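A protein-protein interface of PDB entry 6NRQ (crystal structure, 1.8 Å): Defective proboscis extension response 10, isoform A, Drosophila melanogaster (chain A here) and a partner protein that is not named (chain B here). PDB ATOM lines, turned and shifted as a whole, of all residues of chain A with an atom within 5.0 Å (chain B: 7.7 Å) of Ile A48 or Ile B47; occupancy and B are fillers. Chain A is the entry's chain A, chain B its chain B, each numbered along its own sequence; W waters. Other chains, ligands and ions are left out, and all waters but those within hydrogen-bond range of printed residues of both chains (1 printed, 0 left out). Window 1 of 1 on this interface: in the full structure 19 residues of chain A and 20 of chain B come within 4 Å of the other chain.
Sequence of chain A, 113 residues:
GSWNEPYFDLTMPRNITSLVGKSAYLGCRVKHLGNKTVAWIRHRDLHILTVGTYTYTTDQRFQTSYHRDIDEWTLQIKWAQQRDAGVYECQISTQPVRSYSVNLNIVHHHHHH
Water W1 lies within hydrogen-bond range of a ring nitrogen (NE2) of His A47, the side-chain hydroxyl of Thr A57 and the backbone carbonyl oxygen of Asn B91.
The backbone carbonyl oxygen of Leu A49 sits at hydrogen-bond distance from the backbone NH of Tyr A56 (2.8 Å). O of Ala B46 is in hydrogen-bond range of NE2 of Gln B48 (3.1 Å). O of Leu B40 is in hydrogen-bond range of N of Met B87, 2.8 Å away. N of Lys B41 sits at hydrogen-bond distance from O of Ala B46 (2.8 Å). SD of Met B87 is in hydrogen-bond range of NE2 of Gln B89 (3.7 Å). A ring nitrogen (NE2) of His A47 sits at hydrogen-bond distance from the side-chain hydroxyl (OG1) of Thr A57, at 3.1 Å.
The backbone NH (N) of Ile A48 sits at hydrogen-bond distance from the side-chain amide oxygen (OE1) of Gln B89 (2.7 Å). The backbone carbonyl oxygen of Tyr A56 lies within hydrogen-bond range of the side-chain amide nitrogen of Asn B91 (3.0 Å). OH of Tyr A56 sits at hydrogen-bond distance from O of Gln B89, at 3.0 Å. The backbone carbonyl oxygen (O) of Lys B45 is in hydrogen-bond range of the side-chain amide nitrogen (NE2) of Gln A91, 2.7 Å away. The side-chain hydroxyl of Tyr A56 sits at hydrogen-bond distance from the backbone NH of Gly B38, 3.2 Å away. OE1 of Gln B89 sits at hydrogen-bond distance from ND1 of His A47, 2.8 Å away. The side-chain amide oxygen (OE1) of Gln A91 sits at hydrogen-bond distance from the backbone NH (N) of Ile B47. O of Leu A46 lies within hydrogen-bond range of NE2 of Gln B89 (3.0 Å).
Of the printed residues of chain B, Ile A48 touches Ile B47 (3.8 Å) and Gln B89 (2.7 Å). Of chain A, only Ala A39 (3.5 Å), Ile A41 (3.5 Å), Ile A48 (3.8 Å) and Gln A91 (3.0 Å) come within 4 Å of Ile B47. Of the printed residues of chain A, Gln B89 touches Leu A46, His A47, Ile A48 and Tyr A56. Of the printed residues of chain A, Met B95 touches His A47.
Hydrophobic or aromatic side chains of chain B that line the printed part of chain A: Leu B40, Ile B47, Ile B50, Ile B55, Met B87 and Met B95. Among the printed residues, 22 pairs touch across the chains. Among the printed residues, no Asp or Glu carboxylate lies within 4 Å of a Lys or Arg side-chain nitrogen of the other chain.
Ile A41 touches Lys B45. Ile A41 touches Ile B47. O of Leu A46 touches CD2 of Leu B40, 3.2 Å away. CD2 of Leu A46 touches CD of Lys B45, at 3.7 Å. Leu A46 touches Met B87. Ile B50 touches Val A51 (CD1 to CG2, 3.7 Å). Val A51 touches Ile B55. Tyr A56 touches Val B37. CD1 of Tyr A56 touches CG2 of Ile B50, at 3.6 Å. NE2 of Gln A91 touches CA of Ala B46 (3.6 Å).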
ATOM      1  N   ALA A  39     -35.171  10.428  -9.967  1.00  0.00           N
ATOM      2  CA  ALA A  39     -33.733  10.638 -10.089  1.00  0.00           C
ATOM      3  C   ALA A  39     -33.199  10.031 -11.380  1.00  0.00           C
ATOM      4  O   ALA A  39     -33.730   9.037 -11.885  1.00  0.00           O
ATOM      5  CB  ALA A  39     -32.994  10.034  -8.882  1.00  0.00           C
ATOM      6  N   TRP A  40     -32.128  10.623 -11.915  1.00  0.00           N
ATOM      7  CA  TRP A  40     -31.413  10.046 -13.044  1.00  0.00           C
ATOM      8  C   TRP A  40     -30.018   9.625 -12.609  1.00  0.00           C
ATOM      9  O   TRP A  40     -29.287  10.409 -11.980  1.00  0.00           O
ATOM     10  CB  TRP A  40     -31.317  11.018 -14.218  1.00  0.00           C
ATOM     11  CG  TRP A  40     -32.537  11.091 -15.062  1.00  0.00           C
ATOM     12  CD1 TRP A  40     -33.544  12.019 -14.977  1.00  0.00           C
ATOM     13  CD2 TRP A  40     -32.885  10.212 -16.146  1.00  0.00           C
ATOM     14  NE1 TRP A  40     -34.493  11.763 -15.943  1.00  0.00           N
ATOM     15  CE2 TRP A  40     -34.110  10.668 -16.673  1.00  0.00           C
ATOM     16  CE3 TRP A  40     -32.279   9.077 -16.720  1.00  0.00           C
ATOM     17  CZ2 TRP A  40     -34.748  10.029 -17.746  1.00  0.00           C
ATOM     18  CZ3 TRP A  40     -32.912   8.447 -17.790  1.00  0.00           C
ATOM     19  CH2 TRP A  40     -34.132   8.928 -18.293  1.00  0.00           C
ATOM     20  N   ILE A  41     -29.642   8.400 -12.979  1.00  0.00           N
ATOM     21  CA  ILE A  41     -28.391   7.774 -12.565  1.00  0.00           C
ATOM     22  C   ILE A  41     -27.723   7.169 -13.787  1.00  0.00           C
ATOM     23  O   ILE A  41     -28.394   6.656 -14.689  1.00  0.00           O
ATOM     24  CB  ILE A  41     -28.658   6.674 -11.505  1.00  0.00           C
ATOM     25  CG1 ILE A  41     -29.267   7.269 -10.251  1.00  0.00           C
ATOM     26  CG2 ILE A  41     -27.395   5.891 -11.144  1.00  0.00           C
ATOM     27  CD1 ILE A  41     -30.074   6.207  -9.513  1.00  0.00           C
ATOM     28  N   LEU A  46     -22.599   4.081 -11.736  1.00  0.00           N
ATOM     29  CA  LEU A  46     -23.606   4.377 -10.705  1.00  0.00           C
ATOM     30  C   LEU A  46     -23.518   5.822 -10.211  1.00  0.00           C
ATOM     31  O   LEU A  46     -23.891   6.122  -9.067  1.00  0.00           O
ATOM     32  CB  LEU A  46     -23.517   3.402  -9.521  1.00  0.00           C
ATOM     33  CG  LEU A  46     -23.739   1.923  -9.878  1.00  0.00           C
ATOM     34  CD1 LEU A  46     -23.833   1.050  -8.622  1.00  0.00           C
ATOM     35  CD2 LEU A  46     -24.977   1.795 -10.746  1.00  0.00           C
ATOM     36  N   HIS A  47     -23.063   6.747 -11.064  1.00  0.00           N
ATOM     37  CA  HIS A  47     -23.004   8.150 -10.655  1.00  0.00           C
ATOM     38  C   HIS A  47     -24.412   8.730 -10.639  1.00  0.00           C
ATOM     39  O   HIS A  47     -25.127   8.674 -11.650  1.00  0.00           O
ATOM     40  CB  HIS A  47     -22.106   8.953 -11.598  1.00  0.00           C
ATOM     41  CG  HIS A  47     -21.817  10.352 -11.132  1.00  0.00           C
ATOM     42  ND1 HIS A  47     -21.874  10.727  -9.804  1.00  0.00           N
ATOM     43  CD2 HIS A  47     -21.462  11.464 -11.823  1.00  0.00           C
ATOM     44  CE1 HIS A  47     -21.558  12.008  -9.698  1.00  0.00           C
ATOM     45  NE2 HIS A  47     -21.305  12.478 -10.907  1.00  0.00           N
ATOM     46  N   ILE A  48     -24.808   9.283  -9.492  1.00  0.00           N
ATOM     47  CA  ILE A  48     -26.049  10.045  -9.396  1.00  0.00           C
ATOM     48  C   ILE A  48     -25.907  11.333 -10.190  1.00  0.00           C
ATOM     49  O   ILE A  48     -24.935  12.084 -10.009  1.00  0.00           O
ATOM     50  CB  ILE A  48     -26.381  10.350  -7.925  1.00  0.00           C
ATOM     51  CG1 ILE A  48     -26.661   9.055  -7.142  1.00  0.00           C
ATOM     52  CG2 ILE A  48     -27.603  11.277  -7.831  1.00  0.00           C
ATOM     53  CD1 ILE A  48     -26.525   9.205  -5.643  1.00  0.00           C
ATOM     54  N   LEU A  49     -26.884  11.616 -11.062  1.00  0.00           N
ATOM     55  CA  LEU A  49     -26.828  12.835 -11.877  1.00  0.00           C
ATOM     56  C   LEU A  49     -27.754  13.913 -11.329  1.00  0.00           C
ATOM     57  O   LEU A  49     -27.301  15.002 -10.966  1.00  0.00           O
ATOM     58  CB  LEU A  49     -27.168  12.519 -13.344  1.00  0.00           C
ATOM     59  CG  LEU A  49     -26.301  11.425 -13.976  1.00  0.00           C
ATOM     60  CD1 LEU A  49     -26.875  10.927 -15.315  1.00  0.00           C
ATOM     61  CD2 LEU A  49     -24.864  11.911 -14.164  1.00  0.00           C
ATOM     62  N   THR A  50     -29.049  13.615 -11.235  1.00  0.00           N
ATOM     63  CA  THR A  50     -30.060  14.570 -10.806  1.00  0.00           C
ATOM     64  C   THR A  50     -31.057  13.877  -9.881  1.00  0.00           C
ATOM     65  O   THR A  50     -31.312  12.678 -10.008  1.00  0.00           O
ATOM     66  CB  THR A  50     -30.826  15.191 -11.995  1.00  0.00           C
ATOM     67  OG1 THR A  50     -31.505  14.167 -12.725  1.00  0.00           O
ATOM     68  CG2 THR A  50     -29.866  15.955 -12.949  1.00  0.00           C
ATOM     69  N   VAL A  51     -31.606  14.636  -8.937  1.00  0.00           N
ATOM     70  CA  VAL A  51     -32.747  14.195  -8.134  1.00  0.00           C
ATOM     71  C   VAL A  51     -33.800  15.284  -8.239  1.00  0.00           C
ATOM     72  O   VAL A  51     -33.559  16.418  -7.809  1.00  0.00           O
ATOM     73  CB  VAL A  51     -32.377  13.932  -6.665  1.00  0.00           C
ATOM     74  CG1 VAL A  51     -33.623  13.461  -5.876  1.00  0.00           C
ATOM     75  CG2 VAL A  51     -31.237  12.904  -6.587  1.00  0.00           C
ATOM     76  N   TYR A  56     -26.860  16.829  -8.858  1.00  0.00           N
ATOM     77  CA  TYR A  56     -25.811  16.381  -7.945  1.00  0.00           C
ATOM     78  C   TYR A  56     -24.438  16.393  -8.617  1.00  0.00           C
ATOM     79  O   TYR A  56     -23.476  16.951  -8.073  1.00  0.00           O
ATOM     80  CB  TYR A  56     -26.150  14.990  -7.426  1.00  0.00           C
ATOM     81  CG  TYR A  56     -25.083  14.328  -6.564  1.00  0.00           C
ATOM     82  CD1 TYR A  56     -24.820  14.773  -5.269  1.00  0.00           C
ATOM     83  CD2 TYR A  56     -24.356  13.239  -7.051  1.00  0.00           C
ATOM     84  CE1 TYR A  56     -23.867  14.152  -4.483  1.00  0.00           C
ATOM     85  CE2 TYR A  56     -23.399  12.612  -6.270  1.00  0.00           C
ATOM     86  CZ  TYR A  56     -23.162  13.071  -4.990  1.00  0.00           C
ATOM     87  OH  TYR A  56     -22.210  12.460  -4.214  1.00  0.00           O
ATOM     88  N   THR A  57     -24.335  15.796  -9.806  1.00  0.00           N
ATOM     89  CA  THR A  57     -23.078  15.804 -10.538  1.00  0.00           C
ATOM     90  C   THR A  57     -22.569  17.232 -10.707  1.00  0.00           C
ATOM     91  O   THR A  57     -23.345  18.187 -10.805  1.00  0.00           O
ATOM     92  CB  THR A  57     -23.254  15.116 -11.902  1.00  0.00           C
ATOM     93  OG1 THR A  57     -21.998  15.028 -12.587  1.00  0.00           O
ATOM     94  CG2 THR A  57     -24.248  15.859 -12.775  1.00  0.00           C
ATOM     95  N   GLN A  91     -35.339   6.817 -11.854  1.00  0.00           N
ATOM     96  CA  GLN A  91     -35.544   6.052 -10.626  1.00  0.00           C
ATOM     97  C   GLN A  91     -36.523   6.774  -9.698  1.00  0.00           C
ATOM     98  O   GLN A  91     -36.281   7.922  -9.308  1.00  0.00           O
ATOM     99  CB  GLN A  91     -34.192   5.848  -9.935  1.00  0.00           C
ATOM    100  CG  GLN A  91     -34.173   4.764  -8.930  1.00  0.00           C
ATOM    101  CD  GLN A  91     -32.856   4.687  -8.185  1.00  0.00           C
ATOM    102  OE1 GLN A  91     -32.627   5.429  -7.223  1.00  0.00           O
ATOM    103  NE2 GLN A  91     -31.980   3.787  -8.624  1.00  0.00           N
ATOM    104  N   VAL B  37     -21.721  14.076  -0.148  1.00  0.00           N
ATOM    105  CA  VAL B  37     -21.625  12.623  -0.060  1.00  0.00           C
ATOM    106  C   VAL B  37     -22.983  12.021  -0.391  1.00  0.00           C
ATOM    107  O   VAL B  37     -23.981  12.309   0.280  1.00  0.00           O
ATOM    108  CB  VAL B  37     -21.168  12.174   1.338  1.00  0.00           C
ATOM    109  CG1 VAL B  37     -21.150  10.645   1.409  1.00  0.00           C
ATOM    110  CG2 VAL B  37     -19.809  12.778   1.673  1.00  0.00           C
ATOM    111  N   GLY B  38     -23.020  11.173  -1.411  1.00  0.00           N
ATOM    112  CA  GLY B  38     -24.203  10.385  -1.719  1.00  0.00           C
ATOM    113  C   GLY B  38     -24.020   8.920  -1.374  1.00  0.00           C
ATOM    114  O   GLY B  38     -22.913   8.380  -1.464  1.00  0.00           O
ATOM    115  N   TRP B  39     -25.122   8.265  -0.996  1.00  0.00           N
ATOM    116  CA  TRP B  39     -25.128   6.848  -0.681  1.00  0.00           C
ATOM    117  C   TRP B  39     -26.108   6.148  -1.605  1.00  0.00           C
ATOM    118  O   TRP B  39     -27.233   6.629  -1.807  1.00  0.00           O
ATOM    119  CB  TRP B  39     -25.549   6.597   0.764  1.00  0.00           C
ATOM    120  CG  TRP B  39     -24.552   6.951   1.808  1.00  0.00           C
ATOM    121  CD1 TRP B  39     -24.537   8.081   2.572  1.00  0.00           C
ATOM    122  CD2 TRP B  39     -23.459   6.141   2.263  1.00  0.00           C
ATOM    123  NE1 TRP B  39     -23.498   8.032   3.471  1.00  0.00           N
ATOM    124  CE2 TRP B  39     -22.816   6.855   3.302  1.00  0.00           C
ATOM    125  CE3 TRP B  39     -22.951   4.895   1.883  1.00  0.00           C
ATOM    126  CZ2 TRP B  39     -21.701   6.355   3.977  1.00  0.00           C
ATOM    127  CZ3 TRP B  39     -21.836   4.392   2.556  1.00  0.00           C
ATOM    128  CH2 TRP B  39     -21.218   5.131   3.587  1.00  0.00           C
ATOM    129  N   LEU B  40     -25.701   5.011  -2.156  1.00  0.00           N
ATOM    130  CA  LEU B  40     -26.644   4.227  -2.928  1.00  0.00           C
ATOM    131  C   LEU B  40     -26.362   2.749  -2.720  1.00  0.00           C
ATOM    132  O   LEU B  40     -25.241   2.335  -2.409  1.00  0.00           O
ATOM    133  CB  LEU B  40     -26.620   4.610  -4.419  1.00  0.00           C
ATOM    134  CG  LEU B  40     -25.524   4.202  -5.384  1.00  0.00           C
ATOM    135  CD1 LEU B  40     -25.688   2.760  -5.864  1.00  0.00           C
ATOM    136  CD2 LEU B  40     -25.558   5.163  -6.567  1.00  0.00           C
ATOM    137  N   LYS B  41     -27.394   1.956  -2.922  1.00  0.00           N
ATOM    138  CA  LYS B  41     -27.289   0.510  -2.801  1.00  0.00           C
ATOM    139  C   LYS B  41     -26.844  -0.063  -4.144  1.00  0.00           C
ATOM    140  O   LYS B  41     -27.550   0.083  -5.148  1.00  0.00           O
ATOM    141  CB  LYS B  41     -28.631  -0.075  -2.366  1.00  0.00           C
ATOM    142  CG  LYS B  41     -28.637  -1.586  -2.210  1.00  0.00           C
ATOM    143  CD  LYS B  41     -28.083  -1.994  -0.866  1.00  0.00           C
ATOM    144  CE  LYS B  41     -27.763  -3.496  -0.774  1.00  0.00           C
ATOM    145  NZ  LYS B  41     -28.920  -4.394  -1.053  1.00  0.00           N
ATOM    146  N   THR B  44     -29.265  -2.914  -6.247  1.00  0.00           N
ATOM    147  CA  THR B  44     -30.501  -2.349  -6.773  1.00  0.00           C
ATOM    148  C   THR B  44     -30.309  -0.992  -7.441  1.00  0.00           C
ATOM    149  O   THR B  44     -31.233  -0.520  -8.115  1.00  0.00           O
ATOM    150  CB  THR B  44     -31.542  -2.166  -5.665  1.00  0.00           C
ATOM    151  OG1 THR B  44     -31.028  -1.263  -4.694  1.00  0.00           O
ATOM    152  CG2 THR B  44     -31.913  -3.505  -4.990  1.00  0.00           C
ATOM    153  N   LYS B  45     -29.158  -0.344  -7.237  1.00  0.00           N
ATOM    154  CA  LYS B  45     -28.856   1.010  -7.694  1.00  0.00           C
ATOM    155  C   LYS B  45     -29.694   2.058  -6.976  1.00  0.00           C
ATOM    156  O   LYS B  45     -29.661   3.231  -7.359  1.00  0.00           O
ATOM    157  CB  LYS B  45     -29.021   1.149  -9.218  1.00  0.00           C
ATOM    158  CG  LYS B  45     -28.280   0.072 -10.006  1.00  0.00           C
ATOM    159  CD  LYS B  45     -28.247   0.360 -11.514  1.00  0.00           C
ATOM    160  CE  LYS B  45     -27.398  -0.659 -12.253  1.00  0.00           C
ATOM    161  NZ  LYS B  45     -28.052  -1.984 -12.322  1.00  0.00           N
ATOM    162  N   ALA B  46     -30.433   1.676  -5.928  1.00  0.00           N
ATOM    163  CA  ALA B  46     -31.332   2.608  -5.255  1.00  0.00           C
ATOM    164  C   ALA B  46     -30.562   3.690  -4.503  1.00  0.00           C
ATOM    165  O   ALA B  46     -29.752   3.388  -3.616  1.00  0.00           O
ATOM    166  CB  ALA B  46     -32.236   1.861  -4.280  1.00  0.00           C
ATOM    167  N   ILE B  47     -30.875   4.955  -4.796  1.00  0.00           N
ATOM    168  CA  ILE B  47     -30.255   6.058  -4.059  1.00  0.00           C
ATOM    169  C   ILE B  47     -30.773   6.051  -2.631  1.00  0.00           C
ATOM    170  O   ILE B  47     -31.991   6.040  -2.400  1.00  0.00           O
ATOM    171  CB  ILE B  47     -30.549   7.404  -4.733  1.00  0.00           C
ATOM    172  CG1 ILE B  47     -29.909   7.466  -6.118  1.00  0.00           C
ATOM    173  CG2 ILE B  47     -30.024   8.558  -3.851  1.00  0.00           C
ATOM    174  CD1 ILE B  47     -30.448   8.601  -6.971  1.00  0.00           C
ATOM    175  N   GLN B  48     -29.856   6.058  -1.661  1.00  0.00           N
ATOM    176  CA  GLN B  48     -30.290   6.108  -0.271  1.00  0.00           C
ATOM    177  C   GLN B  48     -30.395   7.539   0.246  1.00  0.00           C
ATOM    178  O   GLN B  48     -31.407   7.907   0.860  1.00  0.00           O
ATOM    179  CB  GLN B  48     -29.333   5.289   0.603  1.00  0.00           C
ATOM    180  CG  GLN B  48     -29.229   3.831   0.141  1.00  0.00           C
ATOM    181  CD  GLN B  48     -30.566   3.088   0.210  1.00  0.00           C
ATOM    182  OE1 GLN B  48     -31.090   2.832   1.289  1.00  0.00           O
ATOM    183  NE2 GLN B  48     -31.112   2.736  -0.947  1.00  0.00           N
ATOM    184  N   ALA B  49     -29.393   8.367  -0.039  1.00  0.00           N
ATOM    185  CA  ALA B  49     -29.254   9.672   0.590  1.00  0.00           C
ATOM    186  C   ALA B  49     -28.242  10.517  -0.179  1.00  0.00           C
ATOM    187  O   ALA B  49     -27.357   9.993  -0.865  1.00  0.00           O
ATOM    188  CB  ALA B  49     -28.811   9.522   2.039  1.00  0.00           C
ATOM    189  N   ILE B  50     -28.381  11.836  -0.047  1.00  0.00           N
ATOM    190  CA  ILE B  50     -27.372  12.799  -0.496  1.00  0.00           C
ATOM    191  C   ILE B  50     -27.232  13.850   0.586  1.00  0.00           C
ATOM    192  O   ILE B  50     -28.219  14.505   0.948  1.00  0.00           O
ATOM    193  CB  ILE B  50     -27.720  13.474  -1.836  1.00  0.00           C
ATOM    194  CG1 ILE B  50     -27.886  12.423  -2.953  1.00  0.00           C
ATOM    195  CG2 ILE B  50     -26.669  14.582  -2.169  1.00  0.00           C
ATOM    196  CD1 ILE B  50     -28.393  13.000  -4.269  1.00  0.00           C
ATOM    197  N   ASN B  53     -29.903  14.684   3.345  1.00  0.00           N
ATOM    198  CA  ASN B  53     -31.254  14.385   2.881  1.00  0.00           C
ATOM    199  C   ASN B  53     -31.366  12.908   2.503  1.00  0.00           C
ATOM    200  O   ASN B  53     -30.697  12.453   1.568  1.00  0.00           O
ATOM    201  CB  ASN B  53     -31.615  15.267   1.686  1.00  0.00           C
ATOM    202  CG  ASN B  53     -31.700  16.733   2.051  1.00  0.00           C
ATOM    203  OD1 ASN B  53     -32.186  17.086   3.121  1.00  0.00           O
ATOM    204  ND2 ASN B  53     -31.200  17.598   1.169  1.00  0.00           N
ATOM    205  N   VAL B  54     -32.204  12.166   3.236  1.00  0.00           N
ATOM    206  CA  VAL B  54     -32.545  10.806   2.834  1.00  0.00           C
ATOM    207  C   VAL B  54     -33.422  10.873   1.597  1.00  0.00           C
ATOM    208  O   VAL B  54     -34.356  11.680   1.518  1.00  0.00           O
ATOM    209  CB  VAL B  54     -33.261  10.061   3.968  1.00  0.00           C
ATOM    210  CG1 VAL B  54     -33.705   8.639   3.499  1.00  0.00           C
ATOM    211  CG2 VAL B  54     -32.375  10.001   5.204  1.00  0.00           C
ATOM    212  N   ILE B  55     -33.123  10.042   0.613  1.00  0.00           N
ATOM    213  CA  ILE B  55     -33.903  10.028  -0.609  1.00  0.00           C
ATOM    214  C   ILE B  55     -34.856   8.841  -0.642  1.00  0.00           C
ATOM    215  O   ILE B  55     -36.018   8.990  -1.026  1.00  0.00           O
ATOM    216  CB  ILE B  55     -32.971  10.048  -1.833  1.00  0.00           C
ATOM    217  CG1 ILE B  55     -32.256  11.417  -1.873  1.00  0.00           C
ATOM    218  CG2 ILE B  55     -33.743   9.823  -3.108  1.00  0.00           C
ATOM    219  CD1 ILE B  55     -31.568  11.713  -3.149  1.00  0.00           C
ATOM    220  N   THR B  56     -34.376   7.668  -0.225  1.00  0.00           N
ATOM    221  CA  THR B  56     -35.221   6.484  -0.248  1.00  0.00           C
ATOM    222  C   THR B  56     -36.374   6.650   0.723  1.00  0.00           C
ATOM    223  O   THR B  56     -36.241   7.253   1.796  1.00  0.00           O
ATOM    224  CB  THR B  56     -34.425   5.223   0.112  1.00  0.00           C
ATOM    225  OG1 THR B  56     -35.307   4.088   0.104  1.00  0.00           O
ATOM    226  CG2 THR B  56     -33.791   5.338   1.494  1.00  0.00           C
ATOM    227  N   HIS B  57     -37.520   6.098   0.343  1.00  0.00           N
ATOM    228  CA  HIS B  57     -38.650   6.085   1.245  1.00  0.00           C
ATOM    229  C   HIS B  57     -38.684   4.834   2.100  1.00  0.00           C
ATOM    230  O   HIS B  57     -39.689   4.580   2.754  1.00  0.00           O
ATOM    231  CB  HIS B  57     -39.950   6.280   0.467  1.00  0.00           C
ATOM    232  CG  HIS B  57     -40.242   7.723   0.202  1.00  0.00           C
ATOM    233  ND1 HIS B  57     -41.297   8.391   0.786  1.00  0.00           N
ATOM    234  CD2 HIS B  57     -39.562   8.651  -0.513  1.00  0.00           C
ATOM    235  CE1 HIS B  57     -41.289   9.653   0.393  1.00  0.00           C
ATOM    236  NE2 HIS B  57     -40.240   9.840  -0.387  1.00  0.00           N
ATOM    237  N   ASN B  58     -37.582   4.078   2.141  1.00  0.00           N
ATOM    238  CA  ASN B  58     -37.346   3.064   3.159  1.00  0.00           C
ATOM    239  C   ASN B  58     -37.306   3.740   4.528  1.00  0.00           C
ATOM    240  O   ASN B  58     -36.364   4.495   4.811  1.00  0.00           O
ATOM    241  CB  ASN B  58     -36.029   2.336   2.882  1.00  0.00           C
ATOM    242  CG  ASN B  58     -35.781   1.178   3.838  1.00  0.00           C
ATOM    243  OD1 ASN B  58     -36.424   1.058   4.880  1.00  0.00           O
ATOM    244  ND2 ASN B  58     -34.845   0.316   3.482  1.00  0.00           N
ATOM    245  N   VAL B  61     -33.951   3.942   6.986  1.00  0.00           N
ATOM    246  CA  VAL B  61     -32.694   4.528   6.525  1.00  0.00           C
ATOM    247  C   VAL B  61     -32.602   5.971   7.027  1.00  0.00           C
ATOM    248  O   VAL B  61     -33.529   6.768   6.833  1.00  0.00           O
ATOM    249  CB  VAL B  61     -32.574   4.467   4.990  1.00  0.00           C
ATOM    250  CG1 VAL B  61     -31.360   5.253   4.508  1.00  0.00           C
ATOM    251  CG2 VAL B  61     -32.511   3.000   4.473  1.00  0.00           C
ATOM    252  N   LEU B  73     -24.198   6.386   6.978  1.00  0.00           N
ATOM    253  CA  LEU B  73     -25.482   5.862   6.534  1.00  0.00           C
ATOM    254  C   LEU B  73     -25.960   4.851   7.572  1.00  0.00           C
ATOM    255  O   LEU B  73     -25.219   3.922   7.917  1.00  0.00           O
ATOM    256  CB  LEU B  73     -25.354   5.208   5.158  1.00  0.00           C
ATOM    257  CG  LEU B  73     -26.631   4.574   4.568  1.00  0.00           C
ATOM    258  CD1 LEU B  73     -27.560   5.669   4.103  1.00  0.00           C
ATOM    259  CD2 LEU B  73     -26.282   3.659   3.405  1.00  0.00           C
ATOM    260  N   MET B  87     -22.558   1.973  -1.598  1.00  0.00           N
ATOM    261  CA  MET B  87     -21.570   2.832  -2.227  1.00  0.00           C
ATOM    262  C   MET B  87     -21.608   4.234  -1.635  1.00  0.00           C
ATOM    263  O   MET B  87     -22.669   4.870  -1.594  1.00  0.00           O
ATOM    264  CB  MET B  87     -21.842   2.901  -3.729  1.00  0.00           C
ATOM    265  CG  MET B  87     -21.005   3.940  -4.454  1.00  0.00           C
ATOM    266  SD  MET B  87     -21.463   4.024  -6.170  1.00  0.00           S
ATOM    267  CE  MET B  87     -20.688   2.530  -6.791  1.00  0.00           C
ATOM    268  N   GLN B  89     -20.293   7.928  -2.451  1.00  0.00           N
ATOM    269  CA  GLN B  89     -20.008   8.624  -3.699  1.00  0.00           C
ATOM    270  C   GLN B  89     -19.774  10.110  -3.426  1.00  0.00           C
ATOM    271  O   GLN B  89     -20.436  10.688  -2.563  1.00  0.00           O
ATOM    272  CB  GLN B  89     -21.199   8.403  -4.624  1.00  0.00           C
ATOM    273  CG  GLN B  89     -21.171   9.022  -5.938  1.00  0.00           C
ATOM    274  CD  GLN B  89     -22.398   8.622  -6.736  1.00  0.00           C
ATOM    275  OE1 GLN B  89     -22.899   9.398  -7.530  1.00  0.00           O
ATOM    276  NE2 GLN B  89     -22.882   7.399  -6.529  1.00  0.00           N
ATOM    277  N   LEU B  90     -18.832  10.731  -4.156  1.00  0.00           N
ATOM    278  CA  LEU B  90     -18.561  12.167  -4.057  1.00  0.00           C
ATOM    279  C   LEU B  90     -18.805  12.800  -5.416  1.00  0.00           C
ATOM    280  O   LEU B  90     -18.387  12.251  -6.435  1.00  0.00           O
ATOM    281  CB  LEU B  90     -17.121  12.462  -3.614  1.00  0.00           C
ATOM    282  CG  LEU B  90     -16.622  11.857  -2.300  1.00  0.00           C
ATOM    283  CD1 LEU B  90     -15.169  12.253  -2.060  1.00  0.00           C
ATOM    284  CD2 LEU B  90     -17.505  12.267  -1.124  1.00  0.00           C
ATOM    285  N   ASN B  91     -19.504  13.932  -5.446  1.00  0.00           N
ATOM    286  CA  ASN B  91     -19.760  14.585  -6.735  1.00  0.00           C
ATOM    287  C   ASN B  91     -18.572  15.408  -7.230  1.00  0.00           C
ATOM    288  O   ASN B  91     -18.735  16.516  -7.757  1.00  0.00           O
ATOM    289  CB  ASN B  91     -21.017  15.444  -6.634  1.00  0.00           C
ATOM    290  CG  ASN B  91     -20.917  16.493  -5.544  1.00  0.00           C
ATOM    291  OD1 ASN B  91     -20.036  16.429  -4.687  1.00  0.00           O
ATOM    292  ND2 ASN B  91     -21.845  17.443  -5.550  1.00  0.00           N
ATOM    293  N   MET B  95     -16.277  11.614 -10.755  1.00  0.00           N
ATOM    294  CA  MET B  95     -16.827  11.116  -9.507  1.00  0.00           C
ATOM    295  C   MET B  95     -15.846  10.158  -8.850  1.00  0.00           C
ATOM    296  O   MET B  95     -15.079   9.462  -9.520  1.00  0.00           O
ATOM    297  CB  MET B  95     -18.156  10.405  -9.758  1.00  0.00           C
ATOM    298  CG  MET B  95     -18.021   9.093 -10.518  1.00  0.00           C
ATOM    299  SD  MET B  95     -18.064   7.672  -9.396  1.00  0.00           S
ATOM    300  CE  MET B  95     -19.735   7.790  -8.840  1.00  0.00           C
HETATM  301  O   HOH W   1     -19.593  14.877 -10.675  1.00  0.00           O
